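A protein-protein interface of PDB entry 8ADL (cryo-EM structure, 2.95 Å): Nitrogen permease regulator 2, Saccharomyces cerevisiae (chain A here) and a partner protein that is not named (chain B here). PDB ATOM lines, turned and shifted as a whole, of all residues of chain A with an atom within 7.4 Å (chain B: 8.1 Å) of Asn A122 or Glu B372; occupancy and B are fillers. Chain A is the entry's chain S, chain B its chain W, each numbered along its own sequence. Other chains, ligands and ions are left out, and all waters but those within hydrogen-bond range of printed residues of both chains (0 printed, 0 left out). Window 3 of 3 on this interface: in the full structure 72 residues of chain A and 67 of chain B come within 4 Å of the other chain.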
ATOM      1  N   TYR A  82     -20.435  -7.212   2.891  1.00  0.00           N
ATOM      2  CA  TYR A  82     -19.382  -6.628   3.703  1.00  0.00           C
ATOM      3  C   TYR A  82     -18.736  -7.684   4.595  1.00  0.00           C
ATOM      4  O   TYR A  82     -19.318  -8.732   4.890  1.00  0.00           O
ATOM      5  CB  TYR A  82     -19.926  -5.478   4.550  1.00  0.00           C
ATOM      6  CG  TYR A  82     -20.774  -4.498   3.772  1.00  0.00           C
ATOM      7  CD1 TYR A  82     -20.188  -3.573   2.916  1.00  0.00           C
ATOM      8  CD2 TYR A  82     -22.158  -4.494   3.894  1.00  0.00           C
ATOM      9  CE1 TYR A  82     -20.956  -2.671   2.202  1.00  0.00           C
ATOM     10  CE2 TYR A  82     -22.935  -3.596   3.184  1.00  0.00           C
ATOM     11  CZ  TYR A  82     -22.330  -2.689   2.340  1.00  0.00           C
ATOM     12  OH  TYR A  82     -23.100  -1.795   1.632  1.00  0.00           O
ATOM     13  N   PHE A 115     -26.651   9.183   3.082  1.00  0.00           N
ATOM     14  CA  PHE A 115     -25.485   8.325   2.897  1.00  0.00           C
ATOM     15  C   PHE A 115     -25.807   6.866   3.194  1.00  0.00           C
ATOM     16  O   PHE A 115     -25.199   5.971   2.598  1.00  0.00           O
ATOM     17  CB  PHE A 115     -24.327   8.819   3.759  1.00  0.00           C
ATOM     18  CG  PHE A 115     -23.488   9.863   3.084  1.00  0.00           C
ATOM     19  CD1 PHE A 115     -22.815   9.568   1.908  1.00  0.00           C
ATOM     20  CD2 PHE A 115     -23.397  11.145   3.602  1.00  0.00           C
ATOM     21  CE1 PHE A 115     -22.047  10.526   1.273  1.00  0.00           C
ATOM     22  CE2 PHE A 115     -22.630  12.108   2.973  1.00  0.00           C
ATOM     23  CZ  PHE A 115     -21.955  11.799   1.807  1.00  0.00           C
ATOM     24  N   LYS A 116     -26.782   6.611   4.073  1.00  0.00           N
ATOM     25  CA  LYS A 116     -27.292   5.255   4.261  1.00  0.00           C
ATOM     26  C   LYS A 116     -27.937   4.737   2.985  1.00  0.00           C
ATOM     27  O   LYS A 116     -27.713   3.587   2.588  1.00  0.00           O
ATOM     28  CB  LYS A 116     -28.301   5.237   5.409  1.00  0.00           C
ATOM     29  CG  LYS A 116     -28.981   3.896   5.632  1.00  0.00           C
ATOM     30  CD  LYS A 116     -29.919   3.954   6.827  1.00  0.00           C
ATOM     31  CE  LYS A 116     -30.376   2.565   7.243  1.00  0.00           C
ATOM     32  NZ  LYS A 116     -31.108   1.869   6.151  1.00  0.00           N
ATOM     33  N   VAL A 117     -28.727   5.589   2.326  1.00  0.00           N
ATOM     34  CA  VAL A 117     -29.363   5.224   1.063  1.00  0.00           C
ATOM     35  C   VAL A 117     -28.317   4.944  -0.010  1.00  0.00           C
ATOM     36  O   VAL A 117     -28.404   3.946  -0.737  1.00  0.00           O
ATOM     37  CB  VAL A 117     -30.334   6.342   0.631  1.00  0.00           C
ATOM     38  CG1 VAL A 117     -30.702   6.211  -0.838  1.00  0.00           C
ATOM     39  CG2 VAL A 117     -31.581   6.319   1.500  1.00  0.00           C
ATOM     40  N   LEU A 118     -27.295   5.799  -0.102  1.00  0.00           N
ATOM     41  CA  LEU A 118     -26.262   5.617  -1.120  1.00  0.00           C
ATOM     42  C   LEU A 118     -25.416   4.372  -0.866  1.00  0.00           C
ATOM     43  O   LEU A 118     -25.062   3.656  -1.812  1.00  0.00           O
ATOM     44  CB  LEU A 118     -25.379   6.860  -1.198  1.00  0.00           C
ATOM     45  CG  LEU A 118     -26.053   8.083  -1.823  1.00  0.00           C
ATOM     46  CD1 LEU A 118     -25.046   9.193  -2.014  1.00  0.00           C
ATOM     47  CD2 LEU A 118     -26.716   7.731  -3.146  1.00  0.00           C
ATOM     48  N   GLU A 119     -25.079   4.096   0.399  1.00  0.00           N
ATOM     49  CA  GLU A 119     -24.317   2.892   0.720  1.00  0.00           C
ATOM     50  C   GLU A 119     -25.143   1.630   0.498  1.00  0.00           C
ATOM     51  O   GLU A 119     -24.610   0.605   0.054  1.00  0.00           O
ATOM     52  CB  GLU A 119     -23.815   2.971   2.164  1.00  0.00           C
ATOM     53  CG  GLU A 119     -23.035   1.752   2.634  1.00  0.00           C
ATOM     54  CD  GLU A 119     -21.759   1.538   1.846  1.00  0.00           C
ATOM     55  OE1 GLU A 119     -20.973   2.498   1.710  1.00  0.00           O
ATOM     56  OE2 GLU A 119     -21.540   0.408   1.362  1.00  0.00           O
ATOM     57  N   GLU A 120     -26.449   1.685   0.776  1.00  0.00           N
ATOM     58  CA  GLU A 120     -27.303   0.535   0.503  1.00  0.00           C
ATOM     59  C   GLU A 120     -27.539   0.346  -0.990  1.00  0.00           C
ATOM     60  O   GLU A 120     -27.788  -0.778  -1.439  1.00  0.00           O
ATOM     61  CB  GLU A 120     -28.638   0.688   1.233  1.00  0.00           C
ATOM     62  CG  GLU A 120     -28.604   0.246   2.686  1.00  0.00           C
ATOM     63  CD  GLU A 120     -29.881   0.587   3.428  1.00  0.00           C
ATOM     64  OE1 GLU A 120     -30.739   1.288   2.850  1.00  0.00           O
ATOM     65  OE2 GLU A 120     -30.029   0.151   4.590  1.00  0.00           O
ATOM     66  N   GLN A 121     -27.466   1.424  -1.769  1.00  0.00           N
ATOM     67  CA  GLN A 121     -27.752   1.350  -3.197  1.00  0.00           C
ATOM     68  C   GLN A 121     -26.532   0.937  -4.018  1.00  0.00           C
ATOM     69  O   GLN A 121     -26.547  -0.110  -4.674  1.00  0.00           O
ATOM     70  CB  GLN A 121     -28.288   2.701  -3.684  1.00  0.00           C
ATOM     71  CG  GLN A 121     -28.745   2.705  -5.131  1.00  0.00           C
ATOM     72  CD  GLN A 121     -28.627   4.072  -5.774  1.00  0.00           C
ATOM     73  OE1 GLN A 121     -28.481   5.084  -5.087  1.00  0.00           O
ATOM     74  NE2 GLN A 121     -28.683   4.109  -7.101  1.00  0.00           N
ATOM     75  N   ASN A 122     -25.464   1.734  -3.978  1.00  0.00           N
ATOM     76  CA  ASN A 122     -24.328   1.520  -4.868  1.00  0.00           C
ATOM     77  C   ASN A 122     -23.011   1.285  -4.140  1.00  0.00           C
ATOM     78  O   ASN A 122     -21.968   1.210  -4.803  1.00  0.00           O
ATOM     79  CB  ASN A 122     -24.187   2.707  -5.830  1.00  0.00           C
ATOM     80  CG  ASN A 122     -23.703   3.968  -5.136  1.00  0.00           C
ATOM     81  OD1 ASN A 122     -22.501   4.223  -5.052  1.00  0.00           O
ATOM     82  ND2 ASN A 122     -24.641   4.763  -4.635  1.00  0.00           N
ATOM     83  N   GLN A 123     -23.039   1.150  -2.807  1.00  0.00           N
ATOM     84  CA  GLN A 123     -21.859   0.901  -1.968  1.00  0.00           C
ATOM     85  C   GLN A 123     -20.791   1.976  -2.188  1.00  0.00           C
ATOM     86  O   GLN A 123     -19.666   1.705  -2.611  1.00  0.00           O
ATOM     87  CB  GLN A 123     -21.293  -0.505  -2.204  1.00  0.00           C
ATOM     88  CG  GLN A 123     -22.094  -1.618  -1.550  1.00  0.00           C
ATOM     89  CD  GLN A 123     -23.155  -2.187  -2.469  1.00  0.00           C
ATOM     90  OE1 GLN A 123     -22.948  -2.308  -3.676  1.00  0.00           O
ATOM     91  NE2 GLN A 123     -24.303  -2.540  -1.901  1.00  0.00           N
ATOM     92  N   LEU A 124     -21.175   3.217  -1.892  1.00  0.00           N
ATOM     93  CA  LEU A 124     -20.326   4.368  -2.180  1.00  0.00           C
ATOM     94  C   LEU A 124     -19.172   4.470  -1.187  1.00  0.00           C
ATOM     95  O   LEU A 124     -17.998   4.466  -1.578  1.00  0.00           O
ATOM     96  CB  LEU A 124     -21.182   5.643  -2.179  1.00  0.00           C
ATOM     97  CG  LEU A 124     -20.629   7.016  -2.572  1.00  0.00           C
ATOM     98  CD1 LEU A 124     -21.743   7.827  -3.193  1.00  0.00           C
ATOM     99  CD2 LEU A 124     -20.076   7.774  -1.379  1.00  0.00           C
ATOM    100  N   LEU A 125     -19.495   4.575   0.105  1.00  0.00           N
ATOM    101  CA  LEU A 125     -18.477   4.804   1.126  1.00  0.00           C
ATOM    102  C   LEU A 125     -17.566   3.598   1.315  1.00  0.00           C
ATOM    103  O   LEU A 125     -16.385   3.765   1.640  1.00  0.00           O
ATOM    104  CB  LEU A 125     -19.143   5.181   2.449  1.00  0.00           C
ATOM    105  CG  LEU A 125     -19.943   6.483   2.420  1.00  0.00           C
ATOM    106  CD1 LEU A 125     -20.734   6.648   3.700  1.00  0.00           C
ATOM    107  CD2 LEU A 125     -19.019   7.668   2.210  1.00  0.00           C
ATOM    108  N   SER A 126     -18.090   2.383   1.130  1.00  0.00           N
ATOM    109  CA  SER A 126     -17.255   1.195   1.290  1.00  0.00           C
ATOM    110  C   SER A 126     -16.247   1.073   0.153  1.00  0.00           C
ATOM    111  O   SER A 126     -15.091   0.699   0.379  1.00  0.00           O
ATOM    112  CB  SER A 126     -18.130  -0.055   1.370  1.00  0.00           C
ATOM    113  OG  SER A 126     -19.089  -0.076   0.327  1.00  0.00           O
ATOM    114  N   LYS A 127     -16.666   1.384  -1.076  1.00  0.00           N
ATOM    115  CA  LYS A 127     -15.747   1.363  -2.206  1.00  0.00           C
ATOM    116  C   LYS A 127     -14.830   2.578  -2.241  1.00  0.00           C
ATOM    117  O   LYS A 127     -13.782   2.527  -2.895  1.00  0.00           O
ATOM    118  CB  LYS A 127     -16.522   1.269  -3.522  1.00  0.00           C
ATOM    119  CG  LYS A 127     -17.108  -0.106  -3.798  1.00  0.00           C
ATOM    120  CD  LYS A 127     -17.408  -0.308  -5.278  1.00  0.00           C
ATOM    121  CE  LYS A 127     -18.198   0.856  -5.862  1.00  0.00           C
ATOM    122  NZ  LYS A 127     -19.553   0.968  -5.255  1.00  0.00           N
ATOM    123  N   ASP A 219     -21.795  12.976  -7.130  1.00  0.00           N
ATOM    124  CA  ASP A 219     -21.907  11.986  -8.196  1.00  0.00           C
ATOM    125  C   ASP A 219     -22.499  12.667  -9.423  1.00  0.00           C
ATOM    126  O   ASP A 219     -22.569  13.898  -9.500  1.00  0.00           O
ATOM    127  CB  ASP A 219     -22.765  10.792  -7.757  1.00  0.00           C
ATOM    128  CG  ASP A 219     -21.966   9.723  -7.047  1.00  0.00           C
ATOM    129  OD1 ASP A 219     -20.795   9.499  -7.421  1.00  0.00           O
ATOM    130  OD2 ASP A 219     -22.516   9.093  -6.121  1.00  0.00           O
ATOM    131  N   GLU A 220     -22.933  11.858 -10.390  1.00  0.00           N
ATOM    132  CA  GLU A 220     -23.613  12.383 -11.566  1.00  0.00           C
ATOM    133  C   GLU A 220     -25.096  12.627 -11.328  1.00  0.00           C
ATOM    134  O   GLU A 220     -25.754  13.227 -12.184  1.00  0.00           O
ATOM    135  CB  GLU A 220     -23.437  11.429 -12.750  1.00  0.00           C
ATOM    136  CG  GLU A 220     -21.991  11.138 -13.117  1.00  0.00           C
ATOM    137  CD  GLU A 220     -21.497   9.823 -12.543  1.00  0.00           C
ATOM    138  OE1 GLU A 220     -22.339   9.001 -12.123  1.00  0.00           O
ATOM    139  OE2 GLU A 220     -20.267   9.610 -12.514  1.00  0.00           O
ATOM    140  N   GLY A 221     -25.633  12.174 -10.197  1.00  0.00           N
ATOM    141  CA  GLY A 221     -27.028  12.389  -9.875  1.00  0.00           C
ATOM    142  C   GLY A 221     -27.257  12.732  -8.419  1.00  0.00           C
ATOM    143  O   GLY A 221     -28.392  12.982  -8.003  1.00  0.00           O
ATOM    144  N   ASN A 222     -26.183  12.790  -7.638  1.00  0.00           N
ATOM    145  CA  ASN A 222     -26.268  13.013  -6.203  1.00  0.00           C
ATOM    146  C   ASN A 222     -25.515  14.277  -5.822  1.00  0.00           C
ATOM    147  O   ASN A 222     -24.426  14.548  -6.339  1.00  0.00           O
ATOM    148  CB  ASN A 222     -25.700  11.823  -5.421  1.00  0.00           C
ATOM    149  CG  ASN A 222     -26.608  10.615  -5.456  1.00  0.00           C
ATOM    150  OD1 ASN A 222     -27.721  10.649  -4.934  1.00  0.00           O
ATOM    151  ND2 ASN A 222     -26.139   9.537  -6.075  1.00  0.00           N
ATOM    152  N   VAL B 358     -38.014   8.798 -17.668  1.00  0.00           N
ATOM    153  CA  VAL B 358     -36.723   8.447 -17.085  1.00  0.00           C
ATOM    154  C   VAL B 358     -36.474   6.950 -17.194  1.00  0.00           C
ATOM    155  O   VAL B 358     -35.513   6.504 -17.831  1.00  0.00           O
ATOM    156  CB  VAL B 358     -36.651   8.919 -15.623  1.00  0.00           C
ATOM    157  CG1 VAL B 358     -35.278   8.636 -15.048  1.00  0.00           C
ATOM    158  CG2 VAL B 358     -36.984  10.394 -15.533  1.00  0.00           C
ATOM    159  N   VAL B 359     -37.333   6.153 -16.564  1.00  0.00           N
ATOM    160  CA  VAL B 359     -37.223   4.701 -16.577  1.00  0.00           C
ATOM    161  C   VAL B 359     -38.429   4.143 -17.314  1.00  0.00           C
ATOM    162  O   VAL B 359     -39.575   4.465 -16.979  1.00  0.00           O
ATOM    163  CB  VAL B 359     -37.137   4.127 -15.152  1.00  0.00           C
ATOM    164  CG1 VAL B 359     -36.928   2.622 -15.195  1.00  0.00           C
ATOM    165  CG2 VAL B 359     -36.019   4.802 -14.372  1.00  0.00           C
ATOM    166  N   HIS B 366     -33.780  -4.204 -10.656  1.00  0.00           N
ATOM    167  CA  HIS B 366     -32.730  -3.278 -11.074  1.00  0.00           C
ATOM    168  C   HIS B 366     -32.894  -1.916 -10.410  1.00  0.00           C
ATOM    169  O   HIS B 366     -32.687  -0.879 -11.046  1.00  0.00           O
ATOM    170  CB  HIS B 366     -32.724  -3.137 -12.593  1.00  0.00           C
ATOM    171  CG  HIS B 366     -32.716  -4.445 -13.320  1.00  0.00           C
ATOM    172  ND1 HIS B 366     -31.733  -5.393 -13.136  1.00  0.00           N
ATOM    173  CD2 HIS B 366     -33.573  -4.964 -14.231  1.00  0.00           C
ATOM    174  CE1 HIS B 366     -31.984  -6.439 -13.904  1.00  0.00           C
ATOM    175  NE2 HIS B 366     -33.095  -6.204 -14.577  1.00  0.00           N
ATOM    176  N   TRP B 367     -33.289  -1.911  -9.130  1.00  0.00           N
ATOM    177  CA  TRP B 367     -33.605  -0.669  -8.426  1.00  0.00           C
ATOM    178  C   TRP B 367     -32.389   0.234  -8.252  1.00  0.00           C
ATOM    179  O   TRP B 367     -32.547   1.455  -8.155  1.00  0.00           O
ATOM    180  CB  TRP B 367     -34.225  -0.981  -7.065  1.00  0.00           C
ATOM    181  CG  TRP B 367     -33.275  -1.584  -6.081  1.00  0.00           C
ATOM    182  CD1 TRP B 367     -32.881  -2.888  -6.011  1.00  0.00           C
ATOM    183  CD2 TRP B 367     -32.601  -0.904  -5.016  1.00  0.00           C
ATOM    184  NE1 TRP B 367     -32.001  -3.062  -4.971  1.00  0.00           N
ATOM    185  CE2 TRP B 367     -31.813  -1.858  -4.344  1.00  0.00           C
ATOM    186  CE3 TRP B 367     -32.586   0.420  -4.567  1.00  0.00           C
ATOM    187  CZ2 TRP B 367     -31.019  -1.532  -3.247  1.00  0.00           C
ATOM    188  CZ3 TRP B 367     -31.797   0.743  -3.478  1.00  0.00           C
ATOM    189  CH2 TRP B 367     -31.025  -0.229  -2.830  1.00  0.00           C
ATOM    190  N   VAL B 368     -31.179  -0.333  -8.221  1.00  0.00           N
ATOM    191  CA  VAL B 368     -29.970   0.487  -8.157  1.00  0.00           C
ATOM    192  C   VAL B 368     -29.828   1.320  -9.426  1.00  0.00           C
ATOM    193  O   VAL B 368     -29.596   2.535  -9.375  1.00  0.00           O
ATOM    194  CB  VAL B 368     -28.733  -0.400  -7.925  1.00  0.00           C
ATOM    195  CG1 VAL B 368     -27.478   0.452  -7.809  1.00  0.00           C
ATOM    196  CG2 VAL B 368     -28.926  -1.262  -6.686  1.00  0.00           C
ATOM    197  N   ASP B 369     -30.003   0.675 -10.583  1.00  0.00           N
ATOM    198  CA  ASP B 369     -29.950   1.383 -11.858  1.00  0.00           C
ATOM    199  C   ASP B 369     -31.112   2.357 -11.989  1.00  0.00           C
ATOM    200  O   ASP B 369     -30.957   3.445 -12.556  1.00  0.00           O
ATOM    201  CB  ASP B 369     -29.950   0.379 -13.013  1.00  0.00           C
ATOM    202  CG  ASP B 369     -30.110   1.042 -14.367  1.00  0.00           C
ATOM    203  OD1 ASP B 369     -29.104   1.550 -14.905  1.00  0.00           O
ATOM    204  OD2 ASP B 369     -31.243   1.056 -14.894  1.00  0.00           O
ATOM    205  N   ILE B 370     -32.283   1.976 -11.467  1.00  0.00           N
ATOM    206  CA  ILE B 370     -33.459   2.845 -11.504  1.00  0.00           C
ATOM    207  C   ILE B 370     -33.211   4.124 -10.709  1.00  0.00           C
ATOM    208  O   ILE B 370     -33.476   5.233 -11.190  1.00  0.00           O
ATOM    209  CB  ILE B 370     -34.695   2.083 -10.989  1.00  0.00           C
ATOM    210  CG1 ILE B 370     -35.158   1.053 -12.023  1.00  0.00           C
ATOM    211  CG2 ILE B 370     -35.821   3.034 -10.637  1.00  0.00           C
ATOM    212  CD1 ILE B 370     -35.909  -0.118 -11.426  1.00  0.00           C
ATOM    213  N   MET B 371     -32.674   3.991  -9.490  1.00  0.00           N
ATOM    214  CA  MET B 371     -32.388   5.164  -8.667  1.00  0.00           C
ATOM    215  C   MET B 371     -31.273   6.010  -9.268  1.00  0.00           C
ATOM    216  O   MET B 371     -31.337   7.245  -9.218  1.00  0.00           O
ATOM    217  CB  MET B 371     -32.025   4.739  -7.243  1.00  0.00           C
ATOM    218  CG  MET B 371     -33.206   4.294  -6.397  1.00  0.00           C
ATOM    219  SD  MET B 371     -34.667   5.325  -6.630  1.00  0.00           S
ATOM    220  CE  MET B 371     -34.156   6.834  -5.813  1.00  0.00           C
ATOM    221  N   GLU B 372     -30.254   5.367  -9.851  1.00  0.00           N
ATOM    222  CA  GLU B 372     -29.168   6.107 -10.489  1.00  0.00           C
ATOM    223  C   GLU B 372     -29.678   6.920 -11.675  1.00  0.00           C
ATOM    224  O   GLU B 372     -29.342   8.103 -11.822  1.00  0.00           O
ATOM    225  CB  GLU B 372     -28.061   5.147 -10.924  1.00  0.00           C
ATOM    226  CG  GLU B 372     -26.928   5.024  -9.915  1.00  0.00           C
ATOM    227  CD  GLU B 372     -25.948   3.922 -10.267  1.00  0.00           C
ATOM    228  OE1 GLU B 372     -26.222   3.161 -11.218  1.00  0.00           O
ATOM    229  OE2 GLU B 372     -24.902   3.819  -9.591  1.00  0.00           O
ATOM    230  N   THR B 373     -30.500   6.298 -12.529  1.00  0.00           N
ATOM    231  CA  THR B 373     -31.076   6.998 -13.673  1.00  0.00           C
ATOM    232  C   THR B 373     -32.011   8.118 -13.229  1.00  0.00           C
ATOM    233  O   THR B 373     -32.010   9.202 -13.825  1.00  0.00           O
ATOM    234  CB  THR B 373     -31.816   6.009 -14.575  1.00  0.00           C
ATOM    235  OG1 THR B 373     -31.028   4.823 -14.731  1.00  0.00           O
ATOM    236  CG2 THR B 373     -32.076   6.622 -15.944  1.00  0.00           C
ATOM    237  N   LEU B 374     -32.805   7.879 -12.178  1.00  0.00           N
ATOM    238  CA  LEU B 374     -33.724   8.901 -11.679  1.00  0.00           C
ATOM    239  C   LEU B 374     -32.959  10.111 -11.159  1.00  0.00           C
ATOM    240  O   LEU B 374     -33.299  11.257 -11.475  1.00  0.00           O
ATOM    241  CB  LEU B 374     -34.616   8.312 -10.581  1.00  0.00           C
ATOM    242  CG  LEU B 374     -35.869   9.070 -10.122  1.00  0.00           C
ATOM    243  CD1 LEU B 374     -36.950   8.085  -9.731  1.00  0.00           C
ATOM    244  CD2 LEU B 374     -35.590   9.999  -8.947  1.00  0.00           C
ATOM    245  N   ARG B 375     -31.902   9.866 -10.382  1.00  0.00           N
ATOM    246  CA  ARG B 375     -31.117  10.958  -9.820  1.00  0.00           C
ATOM    247  C   ARG B 375     -30.357  11.714 -10.905  1.00  0.00           C
ATOM    248  O   ARG B 375     -30.302  12.951 -10.880  1.00  0.00           O
ATOM    249  CB  ARG B 375     -30.167  10.407  -8.759  1.00  0.00           C
ATOM    250  CG  ARG B 375     -30.875   9.952  -7.491  1.00  0.00           C
ATOM    251  CD  ARG B 375     -29.983   9.056  -6.652  1.00  0.00           C
ATOM    252  NE  ARG B 375     -30.073   9.371  -5.231  1.00  0.00           N
ATOM    253  CZ  ARG B 375     -30.502   8.525  -4.303  1.00  0.00           C
ATOM    254  NH1 ARG B 375     -30.873   7.293  -4.608  1.00  0.00           N
ATOM    255  NH2 ARG B 375     -30.554   8.927  -3.035  1.00  0.00           N
ATOM    256  N   GLU B 376     -29.790  10.991 -11.880  1.00  0.00           N
ATOM    257  CA  GLU B 376     -29.071  11.641 -12.974  1.00  0.00           C
ATOM    258  C   GLU B 376     -30.005  12.492 -13.828  1.00  0.00           C
ATOM    259  O   GLU B 376     -29.669  13.630 -14.181  1.00  0.00           O
ATOM    260  CB  GLU B 376     -28.369  10.590 -13.835  1.00  0.00           C
ATOM    261  CG  GLU B 376     -26.931  10.312 -13.437  1.00  0.00           C
ATOM    262  CD  GLU B 376     -26.273   9.275 -14.325  1.00  0.00           C
ATOM    263  OE1 GLU B 376     -26.860   8.927 -15.370  1.00  0.00           O
ATOM    264  OE2 GLU B 376     -25.167   8.807 -13.980  1.00  0.00           O
ATOM    265  N   GLU B 377     -31.191  11.968 -14.155  1.00  0.00           N
ATOM    266  CA  GLU B 377     -32.113  12.729 -14.987  1.00  0.00           C
ATOM    267  C   GLU B 377     -32.723  13.900 -14.230  1.00  0.00           C
ATOM    268  O   GLU B 377     -32.987  14.945 -14.833  1.00  0.00           O
ATOM    269  CB  GLU B 377     -33.208  11.819 -15.540  1.00  0.00           C
ATOM    270  CG  GLU B 377     -32.710  10.829 -16.584  1.00  0.00           C
ATOM    271  CD  GLU B 377     -31.693  11.437 -17.530  1.00  0.00           C
ATOM    272  OE1 GLU B 377     -32.062  12.352 -18.298  1.00  0.00           O
ATOM    273  OE2 GLU B 377     -30.523  11.000 -17.507  1.00  0.00           O
ATOM    274  N   PHE B 378     -32.943  13.761 -12.919  1.00  0.00           N
ATOM    275  CA  PHE B 378     -33.420  14.905 -12.150  1.00  0.00           C
ATOM    276  C   PHE B 378     -32.346  15.977 -12.012  1.00  0.00           C
ATOM    277  O   PHE B 378     -32.668  17.170 -11.971  1.00  0.00           O
ATOM    278  CB  PHE B 378     -33.908  14.459 -10.773  1.00  0.00           C
ATOM    279  CG  PHE B 378     -34.893  15.408 -10.147  1.00  0.00           C
ATOM    280  CD1 PHE B 378     -34.462  16.475  -9.374  1.00  0.00           C
ATOM    281  CD2 PHE B 378     -36.255  15.232 -10.341  1.00  0.00           C
ATOM    282  CE1 PHE B 378     -35.374  17.350  -8.808  1.00  0.00           C
ATOM    283  CE2 PHE B 378     -37.170  16.100  -9.774  1.00  0.00           C
ATOM    284  CZ  PHE B 378     -36.729  17.160  -9.007  1.00  0.00           C
ATOM    285  N   MET B 379     -31.073  15.582 -11.932  1.00  0.00           N
ATOM    286  CA  MET B 379     -30.015  16.586 -11.911  1.00  0.00           C
ATOM    287  C   MET B 379     -29.818  17.233 -13.277  1.00  0.00           C
ATOM    288  O   MET B 379     -29.390  18.390 -13.354  1.00  0.00           O
ATOM    289  CB  MET B 379     -28.709  15.959 -11.425  1.00  0.00           C
ATOM    290  CG  MET B 379     -28.652  15.731  -9.924  1.00  0.00           C
ATOM    291  SD  MET B 379     -28.677  17.256  -8.966  1.00  0.00           S
ATOM    292  CE  MET B 379     -29.504  16.699  -7.478  1.00  0.00           C
ATOM    293  N   ARG B1032     -36.548   7.604 -23.191  1.00  0.00           N
ATOM    294  CA  ARG B1032     -35.325   7.256 -22.474  1.00  0.00           C
ATOM    295  C   ARG B1032     -34.086   7.372 -23.352  1.00  0.00           C
ATOM    296  O   ARG B1032     -33.004   7.701 -22.851  1.00  0.00           O
ATOM    297  CB  ARG B1032     -35.434   5.835 -21.917  1.00  0.00           C
ATOM    298  CG  ARG B1032     -34.462   5.528 -20.793  1.00  0.00           C
ATOM    299  CD  ARG B1032     -34.508   4.057 -20.417  1.00  0.00           C
ATOM    300  NE  ARG B1032     -33.600   3.743 -19.321  1.00  0.00           N
ATOM    301  CZ  ARG B1032     -33.624   2.611 -18.629  1.00  0.00           C
ATOM    302  NH1 ARG B1032     -34.504   1.658 -18.893  1.00  0.00           N
ATOM    303  NH2 ARG B1032     -32.745   2.432 -17.648  1.00  0.00           N
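The backbone carbonyl oxygen (O) of Val B368 is in hydrogen-bond range of the side-chain amide nitrogen (NE2) of Gln A121 (2.9 Å).
The side-chain amide nitrogen of Gln A121 sits close to the backbone NH of Glu B372 (3.4 Å).
The side-chain amide oxygen (OE1) of Gln A121 sits at hydrogen-bond distance from the guanidinium group (NH1) of Arg B375, 3.3 Å away.
NE of Arg B375 sits at hydrogen-bond distance from OD1 of Asn A222 (2.7 Å).
The side-chain carboxylate of Glu A220 lies close to the side-chain carboxylate of Glu B376 (3.4 Å).
The backbone carbonyl oxygen of Arg B375 lies close to the backbone carbonyl oxygen of Gly A221 (3.5 Å).
The side-chain amino group (NZ) of Lys A116 is in salt-bridge range of the side-chain carboxylate (OE2) of Glu A120, at 2.6 Å.
O of Leu A118 is in hydrogen-bond range of ND2 of Asn A122.
NZ of Lys A127 sits at hydrogen-bond distance from O of Asn A122 (2.5 Å).
Of the printed residues of chain B, Val A117 touches Arg B375.
Of the printed residues of chain B, Glu A120 touches Trp B367.
Of the printed residues of chain B, Asn A122 touches Glu B372.
Of the printed residues of chain B, Glu A220 touches Glu B376 (3.4 Å).
Val B359 touches none of the printed residues of chain A.
Printed residues of chain A within 4 Å of Trp B367: Glu A120 and Gln A121.
Ile B370 touches none of the printed residues of chain A.
Of the printed residues of chain A, Glu B372 touches Gln A121 and Asn A122.
Of the printed residues of chain A, Met B379 touches Gly A221 (3.4 Å).
The nearest printed residue of chain B that does not touch Asn A122 is Val B368 (4.4 Å).
Of the 18 printed residues of chain A, 7 touch a printed residue of chain B.
Hydrophobic or aromatic side chains of chain A that line the printed part of chain B: Val A117.
Printed residues of chain B that touch a printed residue of chain A: Trp B367, Val B368, Met B371, Glu B372, Arg B375, Glu B376 and Met B379.
Hydrophobic or aromatic side chains of chain B that line the printed part of chain A: Trp B367, Val B368, Met B371 and Met B379.
Among the printed residues, 13 pairs touch across the chains.
Among the printed residues, no Asp or Glu carboxylate lies within 4 Å of a Lys or Arg side-chain nitrogen of the other chain.
Val A117 touches Arg B375.
Glu A120 touches Trp B367.
CH2 of Trp B367 touches CA of Gln A121 (3.7 Å).
Met B371 touches Gln A121 (CB to NE2, 3.4 Å).
Asn A122 touches Glu B372.
Gly A221 touches Glu B376 (CA to N, 3.7 Å).
Gly A221 touches Met B379.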
